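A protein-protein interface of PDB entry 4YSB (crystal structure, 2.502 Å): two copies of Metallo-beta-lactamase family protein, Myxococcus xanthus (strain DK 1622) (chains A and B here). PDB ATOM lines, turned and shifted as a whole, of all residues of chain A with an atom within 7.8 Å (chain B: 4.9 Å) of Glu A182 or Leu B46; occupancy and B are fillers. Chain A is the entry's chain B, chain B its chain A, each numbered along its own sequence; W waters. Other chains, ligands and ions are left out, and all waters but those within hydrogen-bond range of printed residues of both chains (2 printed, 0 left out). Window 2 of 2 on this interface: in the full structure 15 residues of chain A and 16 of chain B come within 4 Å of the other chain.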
ATOM      1  N   VAL A 133      -8.852   8.032  34.071  1.00  0.00           N
ATOM      2  CA  VAL A 133      -9.636   8.520  32.946  1.00  0.00           C
ATOM      3  C   VAL A 133     -11.089   8.686  33.375  1.00  0.00           C
ATOM      4  O   VAL A 133     -11.787   7.700  33.616  1.00  0.00           O
ATOM      5  CB  VAL A 133      -9.566   7.573  31.736  1.00  0.00           C
ATOM      6  CG1 VAL A 133     -10.398   8.125  30.589  1.00  0.00           C
ATOM      7  CG2 VAL A 133      -8.122   7.368  31.304  1.00  0.00           C
ATOM      8  N   ARG A 134     -11.527   9.940  33.476  1.00  0.00           N
ATOM      9  CA  ARG A 134     -12.876  10.274  33.927  1.00  0.00           C
ATOM     10  C   ARG A 134     -13.177   9.660  35.291  1.00  0.00           C
ATOM     11  O   ARG A 134     -14.259   9.113  35.508  1.00  0.00           O
ATOM     12  CB  ARG A 134     -13.921   9.811  32.907  1.00  0.00           C
ATOM     13  CG  ARG A 134     -13.686  10.319  31.497  1.00  0.00           C
ATOM     14  CD  ARG A 134     -13.711  11.835  31.440  1.00  0.00           C
ATOM     15  NE  ARG A 134     -13.618  12.319  30.066  1.00  0.00           N
ATOM     16  CZ  ARG A 134     -12.474  12.534  29.425  1.00  0.00           C
ATOM     17  NH1 ARG A 134     -11.317  12.309  30.034  1.00  0.00           N
ATOM     18  NH2 ARG A 134     -12.486  12.973  28.173  1.00  0.00           N
ATOM     19  N   PHE A 158      -4.045  19.430  38.451  1.00  0.00           N
ATOM     20  CA  PHE A 158      -4.815  20.296  37.557  1.00  0.00           C
ATOM     21  C   PHE A 158      -4.119  21.627  37.276  1.00  0.00           C
ATOM     22  O   PHE A 158      -4.544  22.380  36.401  1.00  0.00           O
ATOM     23  CB  PHE A 158      -6.210  20.556  38.131  1.00  0.00           C
ATOM     24  CG  PHE A 158      -7.162  19.405  37.959  1.00  0.00           C
ATOM     25  CD1 PHE A 158      -6.797  18.292  37.219  1.00  0.00           C
ATOM     26  CD2 PHE A 158      -8.424  19.441  38.526  1.00  0.00           C
ATOM     27  CE1 PHE A 158      -7.671  17.233  37.056  1.00  0.00           C
ATOM     28  CE2 PHE A 158      -9.304  18.386  38.365  1.00  0.00           C
ATOM     29  CZ  PHE A 158      -8.926  17.281  37.629  1.00  0.00           C
ATOM     30  N   ASP A 162      -2.580  22.451  30.399  1.00  0.00           N
ATOM     31  CA  ASP A 162      -3.771  21.791  29.872  1.00  0.00           C
ATOM     32  C   ASP A 162      -3.444  20.650  28.915  1.00  0.00           C
ATOM     33  O   ASP A 162      -4.085  19.599  28.948  1.00  0.00           O
ATOM     34  CB  ASP A 162      -4.669  22.807  29.163  1.00  0.00           C
ATOM     35  CG  ASP A 162      -5.518  23.611  30.126  1.00  0.00           C
ATOM     36  OD1 ASP A 162      -5.199  23.625  31.334  1.00  0.00           O
ATOM     37  OD2 ASP A 162      -6.504  24.228  29.672  1.00  0.00           O
ATOM     38  N   GLU A 163      -2.441  20.861  28.069  1.00  0.00           N
ATOM     39  CA  GLU A 163      -2.102  19.902  27.023  1.00  0.00           C
ATOM     40  C   GLU A 163      -1.373  18.672  27.561  1.00  0.00           C
ATOM     41  O   GLU A 163      -1.078  17.745  26.807  1.00  0.00           O
ATOM     42  CB  GLU A 163      -1.248  20.577  25.945  1.00  0.00           C
ATOM     43  N   THR A 164      -1.084  18.667  28.858  1.00  0.00           N
ATOM     44  CA  THR A 164      -0.369  17.555  29.477  1.00  0.00           C
ATOM     45  C   THR A 164      -1.162  16.256  29.382  1.00  0.00           C
ATOM     46  O   THR A 164      -2.331  16.204  29.761  1.00  0.00           O
ATOM     47  CB  THR A 164      -0.054  17.837  30.961  1.00  0.00           C
ATOM     48  OG1 THR A 164       0.609  19.102  31.084  1.00  0.00           O
ATOM     49  CG2 THR A 164       0.837  16.742  31.537  1.00  0.00           C
ATOM     50  N   LEU A 165      -0.519  15.214  28.867  1.00  0.00           N
ATOM     51  CA  LEU A 165      -1.143  13.902  28.773  1.00  0.00           C
ATOM     52  C   LEU A 165      -1.141  13.202  30.125  1.00  0.00           C
ATOM     53  O   LEU A 165      -0.176  13.300  30.882  1.00  0.00           O
ATOM     54  CB  LEU A 165      -0.427  13.040  27.733  1.00  0.00           C
ATOM     55  CG  LEU A 165      -0.541  13.502  26.278  1.00  0.00           C
ATOM     56  CD1 LEU A 165       0.289  12.610  25.370  1.00  0.00           C
ATOM     57  CD2 LEU A 165      -1.997  13.517  25.839  1.00  0.00           C
ATOM     58  N   VAL A 166      -2.227  12.497  30.422  1.00  0.00           N
ATOM     59  CA  VAL A 166      -2.344  11.780  31.684  1.00  0.00           C
ATOM     60  C   VAL A 166      -2.438  10.277  31.458  1.00  0.00           C
ATOM     61  O   VAL A 166      -3.392   9.787  30.853  1.00  0.00           O
ATOM     62  CB  VAL A 166      -3.571  12.249  32.483  1.00  0.00           C
ATOM     63  CG1 VAL A 166      -3.762  11.387  33.723  1.00  0.00           C
ATOM     64  CG2 VAL A 166      -3.426  13.714  32.857  1.00  0.00           C
ATOM     65  N   VAL A 177      -5.601   6.789  27.724  1.00  0.00           N
ATOM     66  CA  VAL A 177      -5.016   8.074  28.084  1.00  0.00           C
ATOM     67  C   VAL A 177      -6.062   9.188  28.112  1.00  0.00           C
ATOM     68  O   VAL A 177      -7.056   9.144  27.385  1.00  0.00           O
ATOM     69  CB  VAL A 177      -3.875   8.461  27.104  1.00  0.00           C
ATOM     70  CG1 VAL A 177      -4.431   8.788  25.728  1.00  0.00           C
ATOM     71  CG2 VAL A 177      -3.057   9.626  27.641  1.00  0.00           C
ATOM     72  N   THR A 178      -5.843  10.169  28.980  1.00  0.00           N
ATOM     73  CA  THR A 178      -6.627  11.395  28.986  1.00  0.00           C
ATOM     74  C   THR A 178      -5.673  12.580  29.061  1.00  0.00           C
ATOM     75  O   THR A 178      -4.461  12.418  28.913  1.00  0.00           O
ATOM     76  CB  THR A 178      -7.621  11.441  30.163  1.00  0.00           C
ATOM     77  OG1 THR A 178      -8.275  12.716  30.190  1.00  0.00           O
ATOM     78  CG2 THR A 178      -6.899  11.222  31.482  1.00  0.00           C
ATOM     79  N   SER A 179      -6.213  13.772  29.285  1.00  0.00           N
ATOM     80  CA  SER A 179      -5.376  14.954  29.455  1.00  0.00           C
ATOM     81  C   SER A 179      -5.929  15.846  30.562  1.00  0.00           C
ATOM     82  O   SER A 179      -7.085  15.710  30.961  1.00  0.00           O
ATOM     83  CB  SER A 179      -5.259  15.734  28.141  1.00  0.00           C
ATOM     84  OG  SER A 179      -6.516  16.224  27.712  1.00  0.00           O
ATOM     85  N   ILE A 180      -5.088  16.749  31.057  1.00  0.00           N
ATOM     86  CA  ILE A 180      -5.465  17.652  32.139  1.00  0.00           C
ATOM     87  C   ILE A 180      -6.677  18.501  31.764  1.00  0.00           C
ATOM     88  O   ILE A 180      -7.599  18.668  32.564  1.00  0.00           O
ATOM     89  CB  ILE A 180      -4.292  18.575  32.525  1.00  0.00           C
ATOM     90  CG1 ILE A 180      -3.137  17.751  33.097  1.00  0.00           C
ATOM     91  CG2 ILE A 180      -4.733  19.615  33.539  1.00  0.00           C
ATOM     92  CD1 ILE A 180      -3.482  17.044  34.392  1.00  0.00           C
ATOM     93  N   ALA A 181      -6.672  19.020  30.540  1.00  0.00           N
ATOM     94  CA  ALA A 181      -7.779  19.829  30.042  1.00  0.00           C
ATOM     95  C   ALA A 181      -9.089  19.045  30.068  1.00  0.00           C
ATOM     96  O   ALA A 181     -10.122  19.567  30.479  1.00  0.00           O
ATOM     97  CB  ALA A 181      -7.483  20.321  28.637  1.00  0.00           C
ATOM     98  N   GLU A 182      -9.034  17.790  29.633  1.00  0.00           N
ATOM     99  CA  GLU A 182     -10.208  16.922  29.628  1.00  0.00           C
ATOM    100  C   GLU A 182     -10.775  16.722  31.028  1.00  0.00           C
ATOM    101  O   GLU A 182     -11.984  16.825  31.239  1.00  0.00           O
ATOM    102  CB  GLU A 182      -9.867  15.560  29.018  1.00  0.00           C
ATOM    103  CG  GLU A 182      -9.572  15.587  27.532  1.00  0.00           C
ATOM    104  CD  GLU A 182      -9.062  14.252  27.021  1.00  0.00           C
ATOM    105  OE1 GLU A 182      -7.901  14.196  26.565  1.00  0.00           O
ATOM    106  OE2 GLU A 182      -9.821  13.261  27.077  1.00  0.00           O
ATOM    107  N   GLU A 183      -9.895  16.437  31.982  1.00  0.00           N
ATOM    108  CA  GLU A 183     -10.318  16.112  33.340  1.00  0.00           C
ATOM    109  C   GLU A 183     -10.782  17.342  34.114  1.00  0.00           C
ATOM    110  O   GLU A 183     -11.637  17.241  34.990  1.00  0.00           O
ATOM    111  CB  GLU A 183      -9.184  15.413  34.093  1.00  0.00           C
ATOM    112  CG  GLU A 183      -8.771  14.083  33.479  1.00  0.00           C
ATOM    113  CD  GLU A 183      -9.929  13.105  33.371  1.00  0.00           C
ATOM    114  OE1 GLU A 183      -9.987  12.362  32.369  1.00  0.00           O
ATOM    115  OE2 GLU A 183     -10.777  13.076  34.289  1.00  0.00           O
ATOM    116  N   LYS A 184     -10.221  18.502  33.789  1.00  0.00           N
ATOM    117  CA  LYS A 184     -10.638  19.743  34.432  1.00  0.00           C
ATOM    118  C   LYS A 184     -12.054  20.124  34.009  1.00  0.00           C
ATOM    119  O   LYS A 184     -12.722  20.912  34.681  1.00  0.00           O
ATOM    120  CB  LYS A 184      -9.668  20.880  34.101  1.00  0.00           C
ATOM    121  CG  LYS A 184      -8.350  20.816  34.853  1.00  0.00           C
ATOM    122  CD  LYS A 184      -7.385  21.886  34.367  1.00  0.00           C
ATOM    123  CE  LYS A 184      -7.953  23.282  34.551  1.00  0.00           C
ATOM    124  NZ  LYS A 184      -7.033  24.323  34.010  1.00  0.00           N
ATOM    125  N   ARG A 185     -12.507  19.555  32.898  1.00  0.00           N
ATOM    126  CA  ARG A 185     -13.813  19.890  32.344  1.00  0.00           C
ATOM    127  C   ARG A 185     -14.834  18.766  32.505  1.00  0.00           C
ATOM    128  O   ARG A 185     -16.027  19.027  32.666  1.00  0.00           O
ATOM    129  CB  ARG A 185     -13.684  20.242  30.861  1.00  0.00           C
ATOM    130  CG  ARG A 185     -12.702  21.362  30.557  1.00  0.00           C
ATOM    131  CD  ARG A 185     -12.392  21.419  29.067  1.00  0.00           C
ATOM    132  NE  ARG A 185     -11.269  22.304  28.770  1.00  0.00           N
ATOM    133  CZ  ARG A 185     -10.718  22.433  27.567  1.00  0.00           C
ATOM    134  NH1 ARG A 185     -11.185  21.732  26.542  1.00  0.00           N
ATOM    135  NH2 ARG A 185      -9.697  23.262  27.388  1.00  0.00           N
ATOM    136  N   HIS A 186     -14.374  17.519  32.459  1.00  0.00           N
ATOM    137  CA  HIS A 186     -15.298  16.392  32.351  1.00  0.00           C
ATOM    138  C   HIS A 186     -15.144  15.305  33.417  1.00  0.00           C
ATOM    139  O   HIS A 186     -15.755  14.244  33.300  1.00  0.00           O
ATOM    140  CB  HIS A 186     -15.160  15.753  30.966  1.00  0.00           C
ATOM    141  CG  HIS A 186     -15.327  16.720  29.835  1.00  0.00           C
ATOM    142  ND1 HIS A 186     -16.543  17.279  29.504  1.00  0.00           N
ATOM    143  CD2 HIS A 186     -14.431  17.225  28.954  1.00  0.00           C
ATOM    144  CE1 HIS A 186     -16.388  18.087  28.470  1.00  0.00           C
ATOM    145  NE2 HIS A 186     -15.116  18.074  28.118  1.00  0.00           N
ATOM    146  N   ASN A 187     -14.345  15.553  34.450  1.00  0.00           N
ATOM    147  CA  ASN A 187     -14.243  14.598  35.552  1.00  0.00           C
ATOM    148  C   ASN A 187     -15.508  14.641  36.404  1.00  0.00           C
ATOM    149  O   ASN A 187     -15.802  15.656  37.032  1.00  0.00           O
ATOM    150  CB  ASN A 187     -13.014  14.876  36.420  1.00  0.00           C
ATOM    151  CG  ASN A 187     -12.725  13.752  37.400  1.00  0.00           C
ATOM    152  OD1 ASN A 187     -13.393  13.619  38.425  1.00  0.00           O
ATOM    153  ND2 ASN A 187     -11.718  12.941  37.092  1.00  0.00           N
ATOM    154  N   PRO A 188     -16.256  13.529  36.431  1.00  0.00           N
ATOM    155  CA  PRO A 188     -17.585  13.462  37.054  1.00  0.00           C
ATOM    156  C   PRO A 188     -17.591  13.650  38.573  1.00  0.00           C
ATOM    157  O   PRO A 188     -18.670  13.779  39.152  1.00  0.00           O
ATOM    158  CB  PRO A 188     -18.065  12.052  36.691  1.00  0.00           C
ATOM    159  CG  PRO A 188     -16.818  11.271  36.491  1.00  0.00           C
ATOM    160  CD  PRO A 188     -15.844  12.229  35.875  1.00  0.00           C
ATOM    161  N   ALA A 191     -15.039  18.092  38.664  1.00  0.00           N
ATOM    162  CA  ALA A 191     -15.490  19.230  37.868  1.00  0.00           C
ATOM    163  C   ALA A 191     -16.829  19.755  38.373  1.00  0.00           C
ATOM    164  O   ALA A 191     -17.839  19.052  38.333  1.00  0.00           O
ATOM    165  CB  ALA A 191     -15.590  18.846  36.400  1.00  0.00           C
ATOM    166  N   ILE B   2      -4.785  14.380  16.591  1.00  0.00           N
ATOM    167  CA  ILE B   2      -5.263  13.891  17.878  1.00  0.00           C
ATOM    168  C   ILE B   2      -5.456  12.381  17.813  1.00  0.00           C
ATOM    169  O   ILE B   2      -6.216  11.881  16.985  1.00  0.00           O
ATOM    170  CB  ILE B   2      -6.581  14.569  18.289  1.00  0.00           C
ATOM    171  CG1 ILE B   2      -6.380  16.079  18.429  1.00  0.00           C
ATOM    172  CG2 ILE B   2      -7.103  13.979  19.590  1.00  0.00           C
ATOM    173  CD1 ILE B   2      -7.629  16.823  18.837  1.00  0.00           C
ATOM    174  N   ARG B   4      -6.157   8.616  19.808  1.00  0.00           N
ATOM    175  CA  ARG B   4      -6.657   7.870  20.956  1.00  0.00           C
ATOM    176  C   ARG B   4      -6.832   6.399  20.599  1.00  0.00           C
ATOM    177  O   ARG B   4      -7.466   6.065  19.597  1.00  0.00           O
ATOM    178  CB  ARG B   4      -7.985   8.450  21.449  1.00  0.00           C
ATOM    179  CG  ARG B   4      -7.870   9.806  22.130  1.00  0.00           C
ATOM    180  CD  ARG B   4      -7.064   9.712  23.413  1.00  0.00           C
ATOM    181  NE  ARG B   4      -7.058  10.971  24.154  1.00  0.00           N
ATOM    182  CZ  ARG B   4      -6.192  11.956  23.947  1.00  0.00           C
ATOM    183  NH1 ARG B   4      -5.257  11.833  23.016  1.00  0.00           N
ATOM    184  NH2 ARG B   4      -6.263  13.068  24.669  1.00  0.00           N
ATOM    185  N   LEU B  17      -9.134   6.305  17.306  1.00  0.00           N
ATOM    186  CA  LEU B  17      -9.733   7.603  17.040  1.00  0.00           C
ATOM    187  C   LEU B  17      -8.671   8.591  16.579  1.00  0.00           C
ATOM    188  O   LEU B  17      -7.775   8.954  17.342  1.00  0.00           O
ATOM    189  CB  LEU B  17     -10.443   8.133  18.287  1.00  0.00           C
ATOM    190  CG  LEU B  17     -10.920   9.585  18.242  1.00  0.00           C
ATOM    191  CD1 LEU B  17     -11.941   9.796  17.133  1.00  0.00           C
ATOM    192  CD2 LEU B  17     -11.495   9.990  19.589  1.00  0.00           C
ATOM    193  N   ARG B  24     -11.162  19.712  12.720  1.00  0.00           N
ATOM    194  CA  ARG B  24     -11.798  19.042  13.859  1.00  0.00           C
ATOM    195  C   ARG B  24     -12.625  17.835  13.420  1.00  0.00           C
ATOM    196  O   ARG B  24     -13.539  17.412  14.126  1.00  0.00           O
ATOM    197  CB  ARG B  24     -12.669  20.018  14.654  1.00  0.00           C
ATOM    198  CG  ARG B  24     -11.952  21.299  15.053  1.00  0.00           C
ATOM    199  CD  ARG B  24     -10.616  21.017  15.729  1.00  0.00           C
ATOM    200  NE  ARG B  24     -10.762  20.278  16.979  1.00  0.00           N
ATOM    201  CZ  ARG B  24      -9.755  19.998  17.801  1.00  0.00           C
ATOM    202  NH1 ARG B  24      -8.525  20.398  17.507  1.00  0.00           N
ATOM    203  NH2 ARG B  24      -9.977  19.322  18.920  1.00  0.00           N
ATOM    204  N   MET B  42     -16.154  10.244  23.687  1.00  0.00           N
ATOM    205  CA  MET B  42     -14.755  10.637  23.551  1.00  0.00           C
ATOM    206  C   MET B  42     -14.573  11.648  22.425  1.00  0.00           C
ATOM    207  O   MET B  42     -13.786  12.586  22.543  1.00  0.00           O
ATOM    208  CB  MET B  42     -13.871   9.411  23.302  1.00  0.00           C
ATOM    209  CG  MET B  42     -13.819   8.405  24.450  1.00  0.00           C
ATOM    210  SD  MET B  42     -12.885   8.959  25.895  1.00  0.00           S
ATOM    211  CE  MET B  42     -14.188   9.614  26.940  1.00  0.00           C
ATOM    212  N   VAL B  43     -15.304  11.447  21.332  1.00  0.00           N
ATOM    213  CA  VAL B  43     -15.224  12.338  20.179  1.00  0.00           C
ATOM    214  C   VAL B  43     -15.708  13.741  20.534  1.00  0.00           C
ATOM    215  O   VAL B  43     -15.070  14.737  20.184  1.00  0.00           O
ATOM    216  CB  VAL B  43     -16.052  11.798  18.989  1.00  0.00           C
ATOM    217  CG1 VAL B  43     -16.159  12.843  17.890  1.00  0.00           C
ATOM    218  CG2 VAL B  43     -15.437  10.514  18.453  1.00  0.00           C
ATOM    219  N   ALA B  44     -16.831  13.811  21.240  1.00  0.00           N
ATOM    220  CA  ALA B  44     -17.423  15.086  21.625  1.00  0.00           C
ATOM    221  C   ALA B  44     -16.547  15.846  22.615  1.00  0.00           C
ATOM    222  O   ALA B  44     -16.330  17.049  22.466  1.00  0.00           O
ATOM    223  CB  ALA B  44     -18.809  14.863  22.210  1.00  0.00           C
ATOM    224  N   GLU B  45     -16.043  15.139  23.621  1.00  0.00           N
ATOM    225  CA  GLU B  45     -15.262  15.763  24.685  1.00  0.00           C
ATOM    226  C   GLU B  45     -13.881  16.207  24.212  1.00  0.00           C
ATOM    227  O   GLU B  45     -13.253  17.062  24.834  1.00  0.00           O
ATOM    228  CB  GLU B  45     -15.128  14.808  25.874  1.00  0.00           C
ATOM    229  CG  GLU B  45     -16.433  14.576  26.620  1.00  0.00           C
ATOM    230  CD  GLU B  45     -16.283  13.619  27.786  1.00  0.00           C
ATOM    231  OE1 GLU B  45     -15.162  13.110  28.002  1.00  0.00           O
ATOM    232  OE2 GLU B  45     -17.288  13.375  28.486  1.00  0.00           O
ATOM    233  N   LEU B  46     -13.411  15.624  23.113  1.00  0.00           N
ATOM    234  CA  LEU B  46     -12.156  16.052  22.503  1.00  0.00           C
ATOM    235  C   LEU B  46     -12.408  17.179  21.508  1.00  0.00           C
ATOM    236  O   LEU B  46     -11.494  17.610  20.800  1.00  0.00           O
ATOM    237  CB  LEU B  46     -11.459  14.879  21.808  1.00  0.00           C
ATOM    238  CG  LEU B  46     -10.811  13.820  22.702  1.00  0.00           C
ATOM    239  CD1 LEU B  46     -10.247  12.691  21.857  1.00  0.00           C
ATOM    240  CD2 LEU B  46      -9.724  14.440  23.566  1.00  0.00           C
ATOM    241  N   ASP B  47     -13.653  17.646  21.467  1.00  0.00           N
ATOM    242  CA  ASP B  47     -14.085  18.697  20.549  1.00  0.00           C
ATOM    243  C   ASP B  47     -13.771  18.337  19.103  1.00  0.00           C
ATOM    244  O   ASP B  47     -13.077  19.071  18.398  1.00  0.00           O
ATOM    245  CB  ASP B  47     -13.444  20.036  20.920  1.00  0.00           C
ATOM    246  CG  ASP B  47     -14.080  20.662  22.145  1.00  0.00           C
ATOM    247  OD1 ASP B  47     -15.307  20.504  22.322  1.00  0.00           O
ATOM    248  OD2 ASP B  47     -13.355  21.305  22.933  1.00  0.00           O
ATOM    249  N   LEU B  48     -14.287  17.191  18.676  1.00  0.00           N
ATOM    250  CA  LEU B  48     -14.163  16.748  17.295  1.00  0.00           C
ATOM    251  C   LEU B  48     -15.537  16.370  16.762  1.00  0.00           C
ATOM    252  O   LEU B  48     -16.517  16.350  17.508  1.00  0.00           O
ATOM    253  CB  LEU B  48     -13.203  15.561  17.189  1.00  0.00           C
ATOM    254  CG  LEU B  48     -11.754  15.770  17.638  1.00  0.00           C
ATOM    255  CD1 LEU B  48     -11.014  14.442  17.689  1.00  0.00           C
ATOM    256  CD2 LEU B  48     -11.044  16.739  16.710  1.00  0.00           C
HETATM  257  O   HOH W   1      -9.062  10.671  26.019  1.00  0.00           O
HETATM  258  O   HOH W   2     -14.163  19.526  26.275  1.00  0.00           O
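The side-chain carboxylate (OE1) of Glu B45 lies within salt-bridge range of the guanidinium group (NH2) of Arg A134 (2.7 Å).
The guanidinium group of Arg B4 lies within salt-bridge range of the side-chain carboxylate of Glu A182, at 2.7 Å.
Water W2 bridges NE2 of His A186 and O of Glu B45.
Water W1 lies within hydrogen-bond range of NE of Arg B4, O of Val A177 and OE2 of Glu A182.
OG of Ser A179 lies within hydrogen-bond range of OE1 of Glu A182.
NH2 of Arg B24 sits at hydrogen-bond distance from O of Leu B46, 3.0 Å away.
OE1 of Glu A183 is in salt-bridge range of NH1 of Arg A134 (2.7 Å).
The guanidinium group (NH1) of Arg A134 lies within hydrogen-bond range of the side-chain hydroxyl (OG1) of Thr A178, at 3.1 Å.
The backbone NH (N) of Leu B17 is in hydrogen-bond range of the backbone carbonyl oxygen (O) of Arg B4, at 2.8 Å.
NH2 of Arg A134 lies within salt-bridge range of OE2 of Glu A182.
Among the printed residues, pairs that only touch across the chains: Glu A182 with Leu B46 (3.5 Å), Val A177 with Arg B4 (3.6 Å), His A186 with Glu B45 (3.8 Å) and Arg A134 with Met B42 (3.96 Å).
Glu A182 touches two residues of chain B.
Leu B46 touches one residue of chain A.
Of the printed residues of chain A, Glu B45 touches Arg A134 (2.7 Å) and His A186 (3.8 Å).
Of the printed residues of chain B, Val A177 touches Arg B4.
Printed residues of chain B within 4 Å of Arg A134: Met B42 (3.96 Å) and Glu B45 (2.7 Å).
Val A133 touches none of the printed residues of chain B.
Of the 21 printed residues of chain A, 4 touch a printed residue of chain B.
Along chain A the printed residues that touch a printed residue of chain B span positions 134 to 186.
Of the 11 printed residues of chain B, 4 touch a printed residue of chain A.
Hydrophobic or aromatic side chains of chain B within 4 Å of the printed part of chain A: Met B42 and Leu B46.
Among the printed residues, 6 pairs touch across the chains.
Among the printed residues, Asp or Glu carboxylates within 4 Å of a Lys or Arg side-chain nitrogen of the other chain: Arg A134 with Glu B45 (2.7 Å) and Glu A182 with Arg B4 (2.7 Å).
No position is printed for both chains.
Of the 6 pairs that touch across the chains among the printed residues, none has its exchanged pair printed and touching as well.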
